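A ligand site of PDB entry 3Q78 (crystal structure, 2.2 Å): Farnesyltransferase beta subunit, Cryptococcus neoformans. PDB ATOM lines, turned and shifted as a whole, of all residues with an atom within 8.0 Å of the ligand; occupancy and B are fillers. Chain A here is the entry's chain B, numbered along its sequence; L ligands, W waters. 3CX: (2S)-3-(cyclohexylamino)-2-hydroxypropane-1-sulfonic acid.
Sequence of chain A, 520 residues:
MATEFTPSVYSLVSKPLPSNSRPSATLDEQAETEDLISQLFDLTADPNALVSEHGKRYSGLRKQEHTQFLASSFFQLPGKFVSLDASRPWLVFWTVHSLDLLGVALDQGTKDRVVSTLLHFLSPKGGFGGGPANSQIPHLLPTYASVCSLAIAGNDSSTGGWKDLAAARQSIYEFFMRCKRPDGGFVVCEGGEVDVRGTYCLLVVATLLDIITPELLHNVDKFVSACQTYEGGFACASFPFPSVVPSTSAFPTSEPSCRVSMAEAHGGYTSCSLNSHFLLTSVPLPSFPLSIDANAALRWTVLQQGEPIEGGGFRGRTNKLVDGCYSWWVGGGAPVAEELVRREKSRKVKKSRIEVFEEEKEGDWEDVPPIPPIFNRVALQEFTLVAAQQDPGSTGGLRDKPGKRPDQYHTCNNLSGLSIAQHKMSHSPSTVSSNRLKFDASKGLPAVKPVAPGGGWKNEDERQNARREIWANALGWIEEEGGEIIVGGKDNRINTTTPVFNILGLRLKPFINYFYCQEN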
ATOM      1  N   TYR A  58     -36.205  18.073  -6.653  1.00  0.00           N
ATOM      2  CA  TYR A  58     -35.253  18.659  -5.709  1.00  0.00           C
ATOM      3  C   TYR A  58     -35.986  19.577  -4.731  1.00  0.00           C
ATOM      4  O   TYR A  58     -36.862  20.343  -5.114  1.00  0.00           O
ATOM      5  CB  TYR A  58     -34.140  19.424  -6.446  1.00  0.00           C
ATOM      6  CG  TYR A  58     -33.111  20.038  -5.525  1.00  0.00           C
ATOM      7  CD1 TYR A  58     -32.867  21.406  -5.539  1.00  0.00           C
ATOM      8  CD2 TYR A  58     -32.394  19.259  -4.625  1.00  0.00           C
ATOM      9  CE1 TYR A  58     -31.935  21.976  -4.703  1.00  0.00           C
ATOM     10  CE2 TYR A  58     -31.455  19.824  -3.778  1.00  0.00           C
ATOM     11  CZ  TYR A  58     -31.228  21.188  -3.819  1.00  0.00           C
ATOM     12  OH  TYR A  58     -30.302  21.748  -2.975  1.00  0.00           O
ATOM     13  N   GLY A  60     -34.586  21.843  -2.571  1.00  0.00           N
ATOM     14  CA  GLY A  60     -33.883  23.052  -2.175  1.00  0.00           C
ATOM     15  C   GLY A  60     -34.826  24.240  -2.066  1.00  0.00           C
ATOM     16  O   GLY A  60     -35.779  24.353  -2.837  1.00  0.00           O
ATOM     17  N   LEU A  61     -34.570  25.126  -1.101  1.00  0.00           N
ATOM     18  CA  LEU A  61     -35.384  26.326  -0.956  1.00  0.00           C
ATOM     19  C   LEU A  61     -35.261  27.194  -2.203  1.00  0.00           C
ATOM     20  O   LEU A  61     -34.162  27.639  -2.548  1.00  0.00           O
ATOM     21  CB  LEU A  61     -34.985  27.105   0.300  1.00  0.00           C
ATOM     22  CG  LEU A  61     -35.875  28.280   0.698  1.00  0.00           C
ATOM     23  CD1 LEU A  61     -37.282  27.813   1.041  1.00  0.00           C
ATOM     24  CD2 LEU A  61     -35.261  29.047   1.862  1.00  0.00           C
ATOM     25  N   ILE A 486     -29.224  23.116   9.404  1.00  0.00           N
ATOM     26  CA  ILE A 486     -29.740  23.483   8.098  1.00  0.00           C
ATOM     27  C   ILE A 486     -29.957  22.243   7.228  1.00  0.00           C
ATOM     28  O   ILE A 486     -29.022  21.730   6.621  1.00  0.00           O
ATOM     29  CB  ILE A 486     -28.806  24.461   7.365  1.00  0.00           C
ATOM     30  CG1 ILE A 486     -28.276  25.529   8.336  1.00  0.00           C
ATOM     31  CG2 ILE A 486     -29.511  25.110   6.185  1.00  0.00           C
ATOM     32  CD1 ILE A 486     -29.366  26.381   8.962  1.00  0.00           C
ATOM     33  N   VAL A 487     -31.195  21.759   7.196  1.00  0.00           N
ATOM     34  CA  VAL A 487     -31.526  20.578   6.397  1.00  0.00           C
ATOM     35  C   VAL A 487     -31.329  20.883   4.919  1.00  0.00           C
ATOM     36  O   VAL A 487     -31.852  21.870   4.408  1.00  0.00           O
ATOM     37  CB  VAL A 487     -32.979  20.142   6.631  1.00  0.00           C
ATOM     38  CG1 VAL A 487     -33.327  18.939   5.764  1.00  0.00           C
ATOM     39  CG2 VAL A 487     -33.204  19.813   8.100  1.00  0.00           C
ATOM     40  N   GLY A 488     -30.576  20.026   4.245  1.00  0.00           N
ATOM     41  CA  GLY A 488     -30.373  20.160   2.813  1.00  0.00           C
ATOM     42  C   GLY A 488     -29.160  20.975   2.429  1.00  0.00           C
ATOM     43  O   GLY A 488     -28.819  21.075   1.249  1.00  0.00           O
ATOM     44  N   GLY A 489     -28.492  21.575   3.414  1.00  0.00           N
ATOM     45  CA  GLY A 489     -27.282  22.325   3.149  1.00  0.00           C
ATOM     46  C   GLY A 489     -27.420  23.812   3.352  1.00  0.00           C
ATOM     47  O   GLY A 489     -28.527  24.347   3.423  1.00  0.00           O
ATOM     48  N   LYS A 490     -26.268  24.496   3.420  1.00  0.00           N
ATOM     49  CA  LYS A 490     -26.234  25.909   3.774  1.00  0.00           C
ATOM     50  C   LYS A 490     -26.984  26.836   2.820  1.00  0.00           C
ATOM     51  O   LYS A 490     -27.382  27.928   3.201  1.00  0.00           O
ATOM     52  CB  LYS A 490     -24.785  26.369   3.970  1.00  0.00           C
ATOM     53  CG  LYS A 490     -24.087  25.689   5.134  1.00  0.00           C
ATOM     54  CD  LYS A 490     -22.720  26.299   5.405  1.00  0.00           C
ATOM     55  CE  LYS A 490     -22.092  25.698   6.654  1.00  0.00           C
ATOM     56  NZ  LYS A 490     -20.802  26.369   7.000  1.00  0.00           N
ATOM     57  N   ASP A 491     -27.187  26.408   1.580  1.00  0.00           N
ATOM     58  CA  ASP A 491     -27.922  27.224   0.617  1.00  0.00           C
ATOM     59  C   ASP A 491     -29.388  27.366   1.012  1.00  0.00           C
ATOM     60  O   ASP A 491     -30.080  28.270   0.545  1.00  0.00           O
ATOM     61  CB  ASP A 491     -27.799  26.663  -0.799  1.00  0.00           C
ATOM     62  CG  ASP A 491     -26.477  26.994  -1.442  1.00  0.00           C
ATOM     63  OD1 ASP A 491     -25.951  28.103  -1.208  1.00  0.00           O
ATOM     64  OD2 ASP A 491     -25.952  26.138  -2.179  1.00  0.00           O
ATOM     65  N   ASN A 492     -29.867  26.465   1.876  1.00  0.00           N
ATOM     66  CA  ASN A 492     -31.234  26.538   2.384  1.00  0.00           C
ATOM     67  C   ASN A 492     -31.373  27.476   3.574  1.00  0.00           C
ATOM     68  O   ASN A 492     -32.481  27.758   4.029  1.00  0.00           O
ATOM     69  CB  ASN A 492     -31.741  25.154   2.769  1.00  0.00           C
ATOM     70  CG  ASN A 492     -32.047  24.285   1.576  1.00  0.00           C
ATOM     71  OD1 ASN A 492     -32.259  24.785   0.468  1.00  0.00           O
ATOM     72  ND2 ASN A 492     -32.090  22.982   1.786  1.00  0.00           N
ATOM     73  N   ARG A 493     -30.245  27.944   4.108  1.00  0.00           N
ATOM     74  CA  ARG A 493     -30.254  28.769   5.303  1.00  0.00           C
ATOM     75  C   ARG A 493     -30.951  30.101   5.067  1.00  0.00           C
ATOM     76  O   ARG A 493     -30.622  30.812   4.130  1.00  0.00           O
ATOM     77  CB  ARG A 493     -28.843  29.026   5.810  1.00  0.00           C
ATOM     78  CG  ARG A 493     -28.787  29.629   7.215  1.00  0.00           C
ATOM     79  CD  ARG A 493     -27.491  30.387   7.466  1.00  0.00           C
ATOM     80  NE  ARG A 493     -27.722  31.828   7.401  1.00  0.00           N
ATOM     81  CZ  ARG A 493     -27.866  32.603   8.470  1.00  0.00           C
ATOM     82  NH1 ARG A 493     -27.799  32.086   9.684  1.00  0.00           N
ATOM     83  NH2 ARG A 493     -28.071  33.903   8.316  1.00  0.00           N
HETATM   84  OAA 3CX L   1     -21.688  22.131   2.559  1.00  0.00           O
HETATM   85  OAB 3CX L   1     -22.580  24.216   2.252  1.00  0.00           O
HETATM   86  OAC 3CX L   1     -24.869  24.566   0.210  1.00  0.00           O
HETATM   87  OAD 3CX L   1     -24.076  22.900   2.992  1.00  0.00           O
HETATM   88  CAE 3CX L   1     -26.738  23.704  -6.131  1.00  0.00           C
HETATM   89  CAF 3CX L   1     -25.371  23.791  -5.564  1.00  0.00           C
HETATM   90  CAG 3CX L   1     -27.740  23.976  -5.057  1.00  0.00           C
HETATM   91  CAH 3CX L   1     -25.166  22.780  -4.489  1.00  0.00           C
HETATM   92  CAI 3CX L   1     -27.635  22.999  -3.931  1.00  0.00           C
HETATM   93  CAJ 3CX L   1     -24.878  22.967  -1.558  1.00  0.00           C
HETATM   94  CAK 3CX L   1     -23.103  22.984   0.386  1.00  0.00           C
HETATM   95  NAL 3CX L   1     -25.902  23.622  -2.321  1.00  0.00           N
HETATM   96  CAM 3CX L   1     -24.362  23.568  -0.251  1.00  0.00           C
HETATM   97  CAN 3CX L   1     -26.240  22.740  -3.435  1.00  0.00           C
HETATM   98  SAO 3CX L   1     -22.939  22.779   2.075  1.00  0.00           S
HETATM   99  O   HOH W   1     -26.371  20.245  -0.678  1.00  0.00           O
HETATM  100  O   HOH W   2     -28.090  23.463  -0.209  1.00  0.00           O
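An oxygen (OAC) of the ligand lies within hydrogen-bond range of the backbone NH of Asp 491, at 3.3 Å. OD2 of Asp 491 lies within salt-bridge range of NAL of the ligand, 2.5 Å away. An oxygen (OAD) of the ligand lies within hydrogen-bond range of the backbone NH (N) of Lys 490.
Residues that only touch the ligand: Tyr 58 (3.1 Å) and Gly 489 (3.3 Å). Within 4 Å of the ligand: Tyr 58, Gly 489, Lys 490 and Asp 491. The nearest printed residue that does not touch the ligand is Gly 488 (5.2 Å).
Water W2 bridges O of Gly 488 (2.9 Å) and NAL of the ligand (3.0 Å).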
